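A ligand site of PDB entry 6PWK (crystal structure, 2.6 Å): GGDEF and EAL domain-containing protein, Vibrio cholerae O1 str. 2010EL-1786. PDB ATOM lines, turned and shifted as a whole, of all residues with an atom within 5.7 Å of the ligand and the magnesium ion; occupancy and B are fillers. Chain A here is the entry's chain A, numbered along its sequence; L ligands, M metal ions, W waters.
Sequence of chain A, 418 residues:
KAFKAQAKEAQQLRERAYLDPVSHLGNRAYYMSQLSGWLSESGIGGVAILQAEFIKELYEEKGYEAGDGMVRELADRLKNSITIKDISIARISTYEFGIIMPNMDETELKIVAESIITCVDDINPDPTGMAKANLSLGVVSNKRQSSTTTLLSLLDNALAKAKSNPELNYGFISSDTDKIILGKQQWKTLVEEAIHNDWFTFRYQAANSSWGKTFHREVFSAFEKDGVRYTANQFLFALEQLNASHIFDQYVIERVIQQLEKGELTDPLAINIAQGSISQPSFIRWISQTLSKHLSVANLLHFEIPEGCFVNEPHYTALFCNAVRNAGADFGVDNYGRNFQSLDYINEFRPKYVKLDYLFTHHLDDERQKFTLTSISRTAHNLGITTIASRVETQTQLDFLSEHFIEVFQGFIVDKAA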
ATOM      1  N   ARG A 203      25.281 -10.312   5.069  1.00  0.00           N
ATOM      2  CA  ARG A 203      24.512 -11.539   4.978  1.00  0.00           C
ATOM      3  C   ARG A 203      23.297 -11.456   5.893  1.00  0.00           C
ATOM      4  O   ARG A 203      23.373 -10.849   6.974  1.00  0.00           O
ATOM      5  CB  ARG A 203      25.366 -12.755   5.351  1.00  0.00           C
ATOM      6  CG  ARG A 203      26.501 -13.047   4.379  1.00  0.00           C
ATOM      7  CD  ARG A 203      27.550 -13.976   4.971  1.00  0.00           C
ATOM      8  NE  ARG A 203      26.956 -15.044   5.782  1.00  0.00           N
ATOM      9  CZ  ARG A 203      27.268 -15.259   7.054  1.00  0.00           C
ATOM     10  NH1 ARG A 203      28.167 -14.495   7.663  1.00  0.00           N
ATOM     11  NH2 ARG A 203      26.690 -16.253   7.719  1.00  0.00           N
ATOM     12  N   GLN A 205      20.514 -13.823   7.741  1.00  0.00           N
ATOM     13  CA  GLN A 205      20.094 -15.151   8.162  1.00  0.00           C
ATOM     14  C   GLN A 205      18.749 -15.049   8.878  1.00  0.00           C
ATOM     15  O   GLN A 205      18.634 -14.330   9.875  1.00  0.00           O
ATOM     16  CB  GLN A 205      21.137 -15.809   9.068  1.00  0.00           C
ATOM     17  CG  GLN A 205      20.893 -17.289   9.310  1.00  0.00           C
ATOM     18  CD  GLN A 205      21.915 -17.910  10.232  1.00  0.00           C
ATOM     19  OE1 GLN A 205      22.243 -17.368  11.286  1.00  0.00           O
ATOM     20  NE2 GLN A 205      22.444 -19.066   9.835  1.00  0.00           N
ATOM     21  N   GLU A 218      18.889 -11.713  10.967  1.00  0.00           N
ATOM     22  CA  GLU A 218      20.074 -11.168  11.591  1.00  0.00           C
ATOM     23  C   GLU A 218      21.101 -10.775  10.537  1.00  0.00           C
ATOM     24  O   GLU A 218      21.324 -11.495   9.565  1.00  0.00           O
ATOM     25  CB  GLU A 218      20.691 -12.179  12.567  1.00  0.00           C
ATOM     26  CG  GLU A 218      21.916 -11.657  13.296  1.00  0.00           C
ATOM     27  CD  GLU A 218      22.403 -12.599  14.382  1.00  0.00           C
ATOM     28  OE1 GLU A 218      21.857 -13.719  14.490  1.00  0.00           O
ATOM     29  OE2 GLU A 218      23.332 -12.224  15.122  1.00  0.00           O
ATOM     30  N   VAL A 219      21.727  -9.614  10.740  1.00  0.00           N
ATOM     31  CA  VAL A 219      22.686  -9.055   9.795  1.00  0.00           C
ATOM     32  C   VAL A 219      24.092  -9.408  10.251  1.00  0.00           C
ATOM     33  O   VAL A 219      24.464  -9.165  11.409  1.00  0.00           O
ATOM     34  CB  VAL A 219      22.509  -7.535   9.658  1.00  0.00           C
ATOM     35  CG1 VAL A 219      23.584  -6.954   8.759  1.00  0.00           C
ATOM     36  CG2 VAL A 219      21.119  -7.208   9.142  1.00  0.00           C
ATOM     37  N   PHE A 220      24.883  -9.990   9.345  1.00  0.00           N
ATOM     38  CA  PHE A 220      26.280 -10.293   9.590  1.00  0.00           C
ATOM     39  C   PHE A 220      27.143  -9.454   8.664  1.00  0.00           C
ATOM     40  O   PHE A 220      26.902  -9.406   7.455  1.00  0.00           O
ATOM     41  CB  PHE A 220      26.565 -11.785   9.364  1.00  0.00           C
ATOM     42  CG  PHE A 220      25.848 -12.676  10.329  1.00  0.00           C
ATOM     43  CD1 PHE A 220      25.753 -12.351  11.664  1.00  0.00           C
ATOM     44  CD2 PHE A 220      25.245 -13.847   9.894  1.00  0.00           C
ATOM     45  CE1 PHE A 220      25.085 -13.163  12.556  1.00  0.00           C
ATOM     46  CE2 PHE A 220      24.569 -14.673  10.772  1.00  0.00           C
ATOM     47  CZ  PHE A 220      24.494 -14.329  12.100  1.00  0.00           C
ATOM     48  N   SER A 221      28.144  -8.787   9.240  1.00  0.00           N
ATOM     49  CA  SER A 221      28.991  -7.871   8.486  1.00  0.00           C
ATOM     50  C   SER A 221      30.343  -8.502   8.201  1.00  0.00           C
ATOM     51  O   SER A 221      30.919  -9.180   9.049  1.00  0.00           O
ATOM     52  CB  SER A 221      29.181  -6.558   9.262  1.00  0.00           C
ATOM     53  OG  SER A 221      27.937  -5.907   9.470  1.00  0.00           O
ATOM     54  N   THR A 231      35.994 -11.419   8.506  1.00  0.00           N
ATOM     55  CA  THR A 231      34.769 -11.478   9.296  1.00  0.00           C
ATOM     56  C   THR A 231      34.954 -10.744  10.620  1.00  0.00           C
ATOM     57  O   THR A 231      36.060 -10.363  10.999  1.00  0.00           O
ATOM     58  CB  THR A 231      34.335 -12.925   9.531  1.00  0.00           C
ATOM     59  OG1 THR A 231      35.295 -13.593  10.365  1.00  0.00           O
ATOM     60  CG2 THR A 231      34.221 -13.669   8.207  1.00  0.00           C
ATOM     61  N   ALA A 232      33.832 -10.556  11.330  1.00  0.00           N
ATOM     62  CA  ALA A 232      33.819  -9.639  12.458  1.00  0.00           C
ATOM     63  C   ALA A 232      34.668 -10.139  13.625  1.00  0.00           C
ATOM     64  O   ALA A 232      35.320  -9.335  14.306  1.00  0.00           O
ATOM     65  CB  ALA A 232      32.371  -9.397  12.911  1.00  0.00           C
ATOM     66  N   ASN A 233      34.678 -11.447  13.872  1.00  0.00           N
ATOM     67  CA  ASN A 233      35.462 -11.978  14.978  1.00  0.00           C
ATOM     68  C   ASN A 233      36.963 -11.856  14.767  1.00  0.00           C
ATOM     69  O   ASN A 233      37.731 -12.159  15.683  1.00  0.00           O
ATOM     70  CB  ASN A 233      35.095 -13.446  15.243  1.00  0.00           C
ATOM     71  CG  ASN A 233      33.842 -13.586  16.093  1.00  0.00           C
ATOM     72  OD1 ASN A 233      33.432 -12.647  16.767  1.00  0.00           O
ATOM     73  ND2 ASN A 233      33.247 -14.776  16.080  1.00  0.00           N
ATOM     74  N   LEU A 236      36.985  -7.477  15.820  1.00  0.00           N
ATOM     75  CA  LEU A 236      36.155  -6.809  16.822  1.00  0.00           C
ATOM     76  C   LEU A 236      36.892  -6.635  18.149  1.00  0.00           C
ATOM     77  O   LEU A 236      36.606  -5.681  18.892  1.00  0.00           O
ATOM     78  CB  LEU A 236      34.862  -7.574  17.045  1.00  0.00           C
ATOM     79  CG  LEU A 236      33.680  -7.129  16.177  1.00  0.00           C
ATOM     80  CD1 LEU A 236      32.461  -8.000  16.436  1.00  0.00           C
ATOM     81  CD2 LEU A 236      33.363  -5.663  16.429  1.00  0.00           C
ATOM     82  N   PHE A 248      32.306   1.304  13.980  1.00  0.00           N
ATOM     83  CA  PHE A 248      31.883   0.178  13.153  1.00  0.00           C
ATOM     84  C   PHE A 248      30.379  -0.064  13.273  1.00  0.00           C
ATOM     85  O   PHE A 248      29.711  -0.317  12.258  1.00  0.00           O
ATOM     86  CB  PHE A 248      32.673  -1.069  13.557  1.00  0.00           C
ATOM     87  CG  PHE A 248      32.130  -2.343  13.000  1.00  0.00           C
ATOM     88  CD1 PHE A 248      32.355  -2.692  11.673  1.00  0.00           C
ATOM     89  CD2 PHE A 248      31.401  -3.209  13.798  1.00  0.00           C
ATOM     90  CE1 PHE A 248      31.850  -3.870  11.162  1.00  0.00           C
ATOM     91  CE2 PHE A 248      30.905  -4.388  13.288  1.00  0.00           C
ATOM     92  CZ  PHE A 248      31.129  -4.722  11.974  1.00  0.00           C
ATOM     93  N   ASP A 249      29.839   0.023  14.482  1.00  0.00           N
ATOM     94  CA  ASP A 249      28.409  -0.216  14.666  1.00  0.00           C
ATOM     95  C   ASP A 249      27.569   0.888  14.025  1.00  0.00           C
ATOM     96  O   ASP A 249      26.504   0.607  13.457  1.00  0.00           O
ATOM     97  CB  ASP A 249      28.078  -0.343  16.153  1.00  0.00           C
ATOM     98  CG  ASP A 249      28.368  -1.722  16.704  1.00  0.00           C
ATOM     99  OD1 ASP A 249      28.418  -2.681  15.904  1.00  0.00           O
ATOM    100  OD2 ASP A 249      28.555  -1.853  17.929  1.00  0.00           O
ATOM    101  N   VAL A 252      27.394   0.143  10.273  1.00  0.00           N
ATOM    102  CA  VAL A 252      26.487  -0.967   9.975  1.00  0.00           C
ATOM    103  C   VAL A 252      25.035  -0.521  10.113  1.00  0.00           C
ATOM    104  O   VAL A 252      24.188  -0.836   9.263  1.00  0.00           O
ATOM    105  CB  VAL A 252      26.796  -2.174  10.878  1.00  0.00           C
ATOM    106  CG1 VAL A 252      25.746  -3.257  10.705  1.00  0.00           C
ATOM    107  CG2 VAL A 252      28.192  -2.715  10.570  1.00  0.00           C
ATOM    108  N   ILE A 271      20.339  -6.284  14.255  1.00  0.00           N
ATOM    109  CA  ILE A 271      21.678  -5.718  14.145  1.00  0.00           C
ATOM    110  C   ILE A 271      22.450  -6.038  15.419  1.00  0.00           C
ATOM    111  O   ILE A 271      21.994  -5.727  16.527  1.00  0.00           O
ATOM    112  CB  ILE A 271      21.620  -4.193  13.919  1.00  0.00           C
ATOM    113  CG1 ILE A 271      20.762  -3.860  12.700  1.00  0.00           C
ATOM    114  CG2 ILE A 271      23.024  -3.633  13.759  1.00  0.00           C
ATOM    115  CD1 ILE A 271      20.646  -2.379  12.443  1.00  0.00           C
ATOM    116  N   ASN A 272      23.618  -6.661  15.266  1.00  0.00           N
ATOM    117  CA  ASN A 272      24.475  -6.929  16.409  1.00  0.00           C
ATOM    118  C   ASN A 272      25.158  -5.645  16.873  1.00  0.00           C
ATOM    119  O   ASN A 272      25.586  -4.814  16.062  1.00  0.00           O
ATOM    120  CB  ASN A 272      25.534  -7.969  16.056  1.00  0.00           C
ATOM    121  CG  ASN A 272      24.950  -9.340  15.794  1.00  0.00           C
ATOM    122  OD1 ASN A 272      24.583 -10.066  16.716  1.00  0.00           O
ATOM    123  ND2 ASN A 272      24.869  -9.713  14.517  1.00  0.00           N
ATOM    124  N   ILE A 273      25.262  -5.476  18.188  1.00  0.00           N
ATOM    125  CA  ILE A 273      25.918  -4.330  18.795  1.00  0.00           C
ATOM    126  C   ILE A 273      26.990  -4.837  19.742  1.00  0.00           C
ATOM    127  O   ILE A 273      26.729  -5.707  20.579  1.00  0.00           O
ATOM    128  CB  ILE A 273      24.915  -3.426  19.556  1.00  0.00           C
ATOM    129  CG1 ILE A 273      23.757  -3.013  18.650  1.00  0.00           C
ATOM    130  CG2 ILE A 273      25.627  -2.214  20.120  1.00  0.00           C
ATOM    131  CD1 ILE A 273      24.172  -2.136  17.479  1.00  0.00           C
ATOM    132  N   ALA A 274      28.200  -4.319  19.601  1.00  0.00           N
ATOM    133  CA  ALA A 274      29.279  -4.703  20.497  1.00  0.00           C
ATOM    134  C   ALA A 274      29.118  -4.034  21.857  1.00  0.00           C
ATOM    135  O   ALA A 274      28.440  -3.013  22.000  1.00  0.00           O
ATOM    136  CB  ALA A 274      30.643  -4.343  19.891  1.00  0.00           C
ATOM    137  N   GLU A 304      20.521  -6.428  18.672  1.00  0.00           N
ATOM    138  CA  GLU A 304      20.971  -7.624  19.374  1.00  0.00           C
ATOM    139  C   GLU A 304      22.101  -7.239  20.318  1.00  0.00           C
ATOM    140  O   GLU A 304      23.197  -6.881  19.879  1.00  0.00           O
ATOM    141  CB  GLU A 304      21.410  -8.692  18.378  1.00  0.00           C
ATOM    142  CG  GLU A 304      21.211 -10.119  18.884  1.00  0.00           C
ATOM    143  CD  GLU A 304      20.911 -11.099  17.759  1.00  0.00           C
ATOM    144  OE1 GLU A 304      21.852 -11.748  17.265  1.00  0.00           O
ATOM    145  OE2 GLU A 304      19.731 -11.215  17.374  1.00  0.00           O
ATOM    146  N   ASP A 334      21.768 -11.706  22.981  1.00  0.00           N
ATOM    147  CA  ASP A 334      22.495 -12.492  21.985  1.00  0.00           C
ATOM    148  C   ASP A 334      23.117 -13.773  22.553  1.00  0.00           C
ATOM    149  O   ASP A 334      22.930 -14.850  21.995  1.00  0.00           O
ATOM    150  CB  ASP A 334      23.582 -11.624  21.336  1.00  0.00           C
ATOM    151  CG  ASP A 334      23.970 -12.124  19.950  1.00  0.00           C
ATOM    152  OD1 ASP A 334      23.422 -13.148  19.502  1.00  0.00           O
ATOM    153  OD2 ASP A 334      24.811 -11.462  19.307  1.00  0.00           O
ATOM    154  N   ASN A 335      23.864 -13.665  23.651  1.00  0.00           N
ATOM    155  CA  ASN A 335      24.483 -14.836  24.276  1.00  0.00           C
ATOM    156  C   ASN A 335      23.663 -15.354  25.445  1.00  0.00           C
ATOM    157  O   ASN A 335      24.195 -15.676  26.504  1.00  0.00           O
ATOM    158  CB  ASN A 335      25.900 -14.500  24.745  1.00  0.00           C
ATOM    159  CG  ASN A 335      26.882 -14.403  23.587  1.00  0.00           C
ATOM    160  OD1 ASN A 335      26.700 -15.046  22.556  1.00  0.00           O
ATOM    161  ND2 ASN A 335      27.925 -13.603  23.766  1.00  0.00           N
ATOM    162  N   LYS A 355      18.055 -14.854  22.196  1.00  0.00           N
ATOM    163  CA  LYS A 355      18.719 -15.780  21.296  1.00  0.00           C
ATOM    164  C   LYS A 355      19.687 -16.620  22.115  1.00  0.00           C
ATOM    165  O   LYS A 355      20.623 -16.084  22.716  1.00  0.00           O
ATOM    166  CB  LYS A 355      19.438 -15.035  20.178  1.00  0.00           C
ATOM    167  CG  LYS A 355      19.810 -15.910  18.983  1.00  0.00           C
ATOM    168  CD  LYS A 355      20.159 -15.063  17.765  1.00  0.00           C
ATOM    169  CE  LYS A 355      18.982 -14.197  17.343  1.00  0.00           C
ATOM    170  NZ  LYS A 355      19.281 -13.435  16.098  1.00  0.00           N
ATOM    171  N   TYR A 358      24.967 -20.262  21.561  1.00  0.00           N
ATOM    172  CA  TYR A 358      25.163 -21.322  20.583  1.00  0.00           C
ATOM    173  C   TYR A 358      25.855 -22.547  21.169  1.00  0.00           C
ATOM    174  O   TYR A 358      25.880 -23.588  20.507  1.00  0.00           O
ATOM    175  CB  TYR A 358      25.966 -20.791  19.383  1.00  0.00           C
ATOM    176  CG  TYR A 358      27.454 -20.652  19.610  1.00  0.00           C
ATOM    177  CD1 TYR A 358      27.986 -19.486  20.153  1.00  0.00           C
ATOM    178  CD2 TYR A 358      28.335 -21.666  19.244  1.00  0.00           C
ATOM    179  CE1 TYR A 358      29.357 -19.346  20.341  1.00  0.00           C
ATOM    180  CE2 TYR A 358      29.695 -21.533  19.438  1.00  0.00           C
ATOM    181  CZ  TYR A 358      30.196 -20.373  19.986  1.00  0.00           C
ATOM    182  OH  TYR A 358      31.557 -20.247  20.174  1.00  0.00           O
ATOM    183  N   SER A 390      20.093 -20.803  18.396  1.00  0.00           N
ATOM    184  CA  SER A 390      21.148 -20.157  17.618  1.00  0.00           C
ATOM    185  C   SER A 390      22.109 -21.188  17.047  1.00  0.00           C
ATOM    186  O   SER A 390      22.495 -22.142  17.726  1.00  0.00           O
ATOM    187  CB  SER A 390      21.916 -19.151  18.488  1.00  0.00           C
ATOM    188  OG  SER A 390      22.965 -18.536  17.761  1.00  0.00           O
ATOM    189  N   ARG A 391      22.490 -20.962  15.786  1.00  0.00           N
ATOM    190  CA  ARG A 391      23.536 -21.740  15.112  1.00  0.00           C
ATOM    191  C   ARG A 391      23.191 -23.231  15.053  1.00  0.00           C
ATOM    192  O   ARG A 391      24.019 -24.097  15.355  1.00  0.00           O
ATOM    193  CB  ARG A 391      24.903 -21.495  15.776  1.00  0.00           C
ATOM    194  CG  ARG A 391      25.608 -20.265  15.198  1.00  0.00           C
ATOM    195  CD  ARG A 391      26.266 -19.371  16.236  1.00  0.00           C
ATOM    196  NE  ARG A 391      27.663 -19.733  16.471  1.00  0.00           N
ATOM    197  CZ  ARG A 391      28.609 -18.860  16.834  1.00  0.00           C
ATOM    198  NH1 ARG A 391      28.308 -17.579  16.980  1.00  0.00           N
ATOM    199  NH2 ARG A 391      29.849 -19.270  17.021  1.00  0.00           N
ATOM    200  N   VAL A 392      21.959 -23.518  14.648  1.00  0.00           N
ATOM    201  CA  VAL A 392      21.494 -24.891  14.504  1.00  0.00           C
ATOM    202  C   VAL A 392      21.969 -25.432  13.159  1.00  0.00           C
ATOM    203  O   VAL A 392      21.642 -24.875  12.102  1.00  0.00           O
ATOM    204  CB  VAL A 392      19.965 -24.963  14.609  1.00  0.00           C
ATOM    205  CG1 VAL A 392      19.510 -26.409  14.750  1.00  0.00           C
ATOM    206  CG2 VAL A 392      19.474 -24.122  15.774  1.00  0.00           C
ATOM    207  N   GLU A 393      22.747 -26.514  13.201  1.00  0.00           N
ATOM    208  CA  GLU A 393      23.356 -27.104  12.014  1.00  0.00           C
ATOM    209  C   GLU A 393      22.712 -28.396  11.563  1.00  0.00           C
ATOM    210  O   GLU A 393      22.625 -28.643  10.354  1.00  0.00           O
ATOM    211  CB  GLU A 393      24.854 -27.375  12.259  1.00  0.00           C
ATOM    212  CG  GLU A 393      25.678 -26.175  12.600  1.00  0.00           C
ATOM    213  CD  GLU A 393      27.165 -26.467  12.546  1.00  0.00           C
ATOM    214  OE1 GLU A 393      27.888 -25.804  11.770  1.00  0.00           O
ATOM    215  OE2 GLU A 393      27.618 -27.377  13.270  1.00  0.00           O
ATOM    216  N   GLN A 410      17.346 -20.660  14.199  1.00  0.00           N
ATOM    217  CA  GLN A 410      18.246 -19.977  13.275  1.00  0.00           C
ATOM    218  C   GLN A 410      19.495 -20.819  13.075  1.00  0.00           C
ATOM    219  O   GLN A 410      19.982 -21.445  14.023  1.00  0.00           O
ATOM    220  CB  GLN A 410      18.614 -18.574  13.791  1.00  0.00           C
ATOM    221  CG  GLN A 410      19.401 -17.722  12.815  1.00  0.00           C
ATOM    222  CD  GLN A 410      19.726 -16.337  13.364  1.00  0.00           C
ATOM    223  OE1 GLN A 410      19.209 -15.930  14.402  1.00  0.00           O
ATOM    224  NE2 GLN A 410      20.603 -15.616  12.670  1.00  0.00           N
ATOM    225  N   GLY A 411      20.007 -20.841  11.865  1.00  0.00           N
ATOM    226  CA  GLY A 411      21.206 -21.596  11.575  1.00  0.00           C
ATOM    227  C   GLY A 411      21.209 -22.089  10.137  1.00  0.00           C
ATOM    228  O   GLY A 411      20.307 -21.802   9.351  1.00  0.00           O
ATOM    229  N   PHE A 412      22.250 -22.870   9.819  1.00  0.00           N
ATOM    230  CA  PHE A 412      22.426 -23.348   8.454  1.00  0.00           C
ATOM    231  C   PHE A 412      21.397 -24.403   8.083  1.00  0.00           C
ATOM    232  O   PHE A 412      21.070 -24.550   6.893  1.00  0.00           O
ATOM    233  CB  PHE A 412      23.849 -23.902   8.285  1.00  0.00           C
ATOM    234  CG  PHE A 412      24.925 -22.860   8.385  1.00  0.00           C
ATOM    235  CD1 PHE A 412      24.663 -21.536   8.054  1.00  0.00           C
ATOM    236  CD2 PHE A 412      26.192 -23.189   8.818  1.00  0.00           C
ATOM    237  CE1 PHE A 412      25.648 -20.570   8.143  1.00  0.00           C
ATOM    238  CE2 PHE A 412      27.188 -22.224   8.908  1.00  0.00           C
ATOM    239  CZ  PHE A 412      26.915 -20.914   8.578  1.00  0.00           C
ATOM    240  N   ILE A 413      20.874 -25.143   9.055  1.00  0.00           N
ATOM    241  CA  ILE A 413      19.869 -26.159   8.747  1.00  0.00           C
ATOM    242  C   ILE A 413      18.515 -25.542   8.434  1.00  0.00           C
ATOM    243  O   ILE A 413      17.709 -26.145   7.723  1.00  0.00           O
ATOM    244  CB  ILE A 413      19.746 -27.181   9.879  1.00  0.00           C
ATOM    245  CG1 ILE A 413      19.090 -28.463   9.354  1.00  0.00           C
ATOM    246  CG2 ILE A 413      18.968 -26.608  11.057  1.00  0.00           C
ATOM    247  CD1 ILE A 413      18.309 -29.234  10.389  1.00  0.00           C
HETATM  248  P1  LIG L   1      26.886 -14.078  16.411  1.00  0.00           P
HETATM  249  O1  LIG L   1      25.872 -13.130  16.997  1.00  0.00           O
HETATM  250  O2  LIG L   1      26.771 -15.336  17.220  1.00  0.00           O
HETATM  251  O3  LIG L   1      26.486 -14.524  14.888  1.00  0.00           O
HETATM  252  C1  LIG L   1      26.416 -15.882  14.604  1.00  0.00           C
HETATM  253  C2  LIG L   1      27.789 -16.262  13.968  1.00  0.00           C
HETATM  254  O4  LIG L   1      27.844 -17.548  13.762  1.00  0.00           O
HETATM  255  C3  LIG L   1      27.920 -15.672  12.555  1.00  0.00           C
HETATM  256  O5  LIG L   1      29.219 -15.781  12.213  1.00  0.00           O
HETATM  257  C4  LIG L   1      27.127 -16.695  11.734  1.00  0.00           C
HETATM  258  O6  LIG L   1      27.464 -16.566  10.290  1.00  0.00           O
HETATM  259  C5  LIG L   1      27.675 -17.791  12.175  1.00  0.00           C
HETATM  260  N1  LIG L   1      26.985 -19.055  12.087  1.00  0.00           N
HETATM  261  C6  LIG L   1      25.735 -18.609  11.811  1.00  0.00           C
HETATM  262  N2  LIG L   1      24.939 -19.708  11.708  1.00  0.00           N
HETATM  263  C7  LIG L   1      25.681 -20.791  11.917  1.00  0.00           C
HETATM  264  C8  LIG L   1      25.388 -22.299  11.943  1.00  0.00           C
HETATM  265  O7  LIG L   1      24.304 -22.724  11.740  1.00  0.00           O
HETATM  266  N3  LIG L   1      26.447 -23.223  12.222  1.00  0.00           N
HETATM  267  C9  LIG L   1      27.787 -22.765  12.483  1.00  0.00           C
HETATM  268  N4  LIG L   1      28.907 -23.668  12.773  1.00  0.00           N
HETATM  269  N5  LIG L   1      28.029 -21.341  12.458  1.00  0.00           N
HETATM  270  C10 LIG L   1      26.941 -20.368  12.166  1.00  0.00           C
HETATM  271  P2  LIG L   1      29.863 -14.347  11.671  1.00  0.00           P
HETATM  272  O8  LIG L   1      29.371 -13.796  10.364  1.00  0.00           O
HETATM  273  O9  LIG L   1      31.337 -14.608  11.457  1.00  0.00           O
HETATM  274  O10 LIG L   1      29.680 -13.389  13.000  1.00  0.00           O
HETATM  275  C11 LIG L   1      30.578 -13.709  14.024  1.00  0.00           C
HETATM  276  C12 LIG L   1      30.446 -12.747  15.136  1.00  0.00           C
HETATM  277  O11 LIG L   1      30.869 -11.573  14.756  1.00  0.00           O
HETATM  278  C13 LIG L   1      28.828 -12.580  15.571  1.00  0.00           C
HETATM  279  O12 LIG L   1      28.463 -13.595  16.615  1.00  0.00           O
HETATM  280  C14 LIG L   1      28.725 -11.446  16.026  1.00  0.00           C
HETATM  281  O13 LIG L   1      29.000 -11.461  17.507  1.00  0.00           O
HETATM  282  C15 LIG L   1      29.846 -10.575  15.238  1.00  0.00           C
HETATM  283  N6  LIG L   1      29.294  -9.922  14.238  1.00  0.00           N
HETATM  284  C16 LIG L   1      28.965 -10.355  13.012  1.00  0.00           C
HETATM  285  N7  LIG L   1      28.437  -9.295  12.369  1.00  0.00           N
HETATM  286  C17 LIG L   1      28.446  -8.250  13.198  1.00  0.00           C
HETATM  287  C18 LIG L   1      27.979  -6.811  13.024  1.00  0.00           C
HETATM  288  O14 LIG L   1      27.505  -6.482  11.992  1.00  0.00           O
HETATM  289  N8  LIG L   1      28.102  -5.865  14.099  1.00  0.00           N
HETATM  290  C19 LIG L   1      28.674  -6.267  15.346  1.00  0.00           C
HETATM  291  N9  LIG L   1      28.797  -5.314  16.427  1.00  0.00           N
HETATM  292  N10 LIG L   1      29.114  -7.658  15.492  1.00  0.00           N
HETATM  293  C20 LIG L   1      28.985  -8.635  14.376  1.00  0.00           C
HETATM  294 MG    MG M   1      23.967 -12.211  17.335  1.00  0.00          MG
HETATM  295  O   HOH W   1      24.889  -6.961  12.933  1.00  0.00           O
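A nitrogen (N9) of the ligand is in hydrogen-bond range of the backbone carbonyl oxygen of Asn 272.
N4 of the ligand is in hydrogen-bond range of OE1 of Glu 393 (2.6 Å).
N7 of the ligand sits at hydrogen-bond distance from N of Ser 221 (3.2 Å).
OG of Ser 221 is in hydrogen-bond range of O14 of the ligand, 2.6 Å away.
An oxygen (O8) of the ligand lies within salt-bridge range of the guanidinium group (NH1) of Arg 203, 3.0 Å away.
The side-chain carboxylate of Asp 249 lies within hydrogen-bond range of a nitrogen (N9) of the ligand (2.7 Å).
The guanidinium group (NH1) of Arg 391 lies within salt-bridge range of an oxygen (O2) of the ligand (2.7 Å).
An oxygen (O7) of the ligand is in hydrogen-bond range of the backbone NH of Phe 412 (2.8 Å).
The side-chain amide nitrogen of Gln 205 lies within hydrogen-bond range of a nitrogen (N2) of the ligand, at 3.2 Å.
O11 of the ligand sits close to OD1 of Asn 233.
The backbone carbonyl oxygen of Glu 304 lies within hydrogen-bond range of the backbone NH of Ile 273 (3.0 Å).
N of Glu 304 sits at hydrogen-bond distance from O of Ile 271.
The backbone carbonyl oxygen of Gln 205 is in hydrogen-bond range of the backbone NH of Glu 218, at 2.8 Å.
The backbone carbonyl oxygen of Arg 203 is in hydrogen-bond range of the backbone NH of Phe 220 (2.9 Å).
The side-chain carboxylate of Asp 249 lies within hydrogen-bond range of the backbone NH of Ala 274 (3.0 Å).
The backbone NH (N) of Phe 412 sits at hydrogen-bond distance from the backbone carbonyl oxygen (O) of Val 392 (3.1 Å).
OE1 of Gln 205 is in hydrogen-bond range of NE2 of Gln 410, 2.8 Å away.
The backbone carbonyl oxygen (O) of Val 392 is in hydrogen-bond range of the backbone NH (N) of Ile 413.
N of Ala 274 sits close to N9 of the ligand (3.4 Å).
O of Val 392 sits close to O7 of the ligand.
Merely in contact with the ligand: Phe 220 (3.0 Å), Thr 231 (3.9 Å), Ala 232 (3.2 Å), Leu 236 (3.5 Å), Phe 248 (3.3 Å), Val 252 (3.9 Å), Ile 273 (3.8 Å) and Gly 411 (3.3 Å).
Hydrophobic or aromatic side chains that line the ligand: Phe 220, Ala 232, Leu 236, Phe 248, Val 252 and Phe 412.
Of the 30 residues printed, 21 come within 4 Å of the ligand.
The nearest printed residue that does not touch the ligand is Val 219 (4.1 Å).
Four residues have an atom within 4 Å of the magnesium ion: Glu 218, Asn 272, Glu 304 and Asp 334.
Along chain A the residues within 4 Å of the magnesium ion span positions 218 to 334.
The magnesium ion is bound by O1 of the ligand (2.1 Å), OE1 of Glu 304 (2.2 Å), OD2 of Asp 334 (2.3 Å), OE2 of Glu 218 (2.3 Å), OD1 of Asn 272 (2.3 Å) and OD1 of Asp 334 (2.4 Å).
The magnesium ion has six donor atoms within binding distance.
Water W1 lies within hydrogen-bond range of N of Asn 272 (2.7 Å), O of Val 219 (2.7 Å) and O14 of the ligand (2.8 Å).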
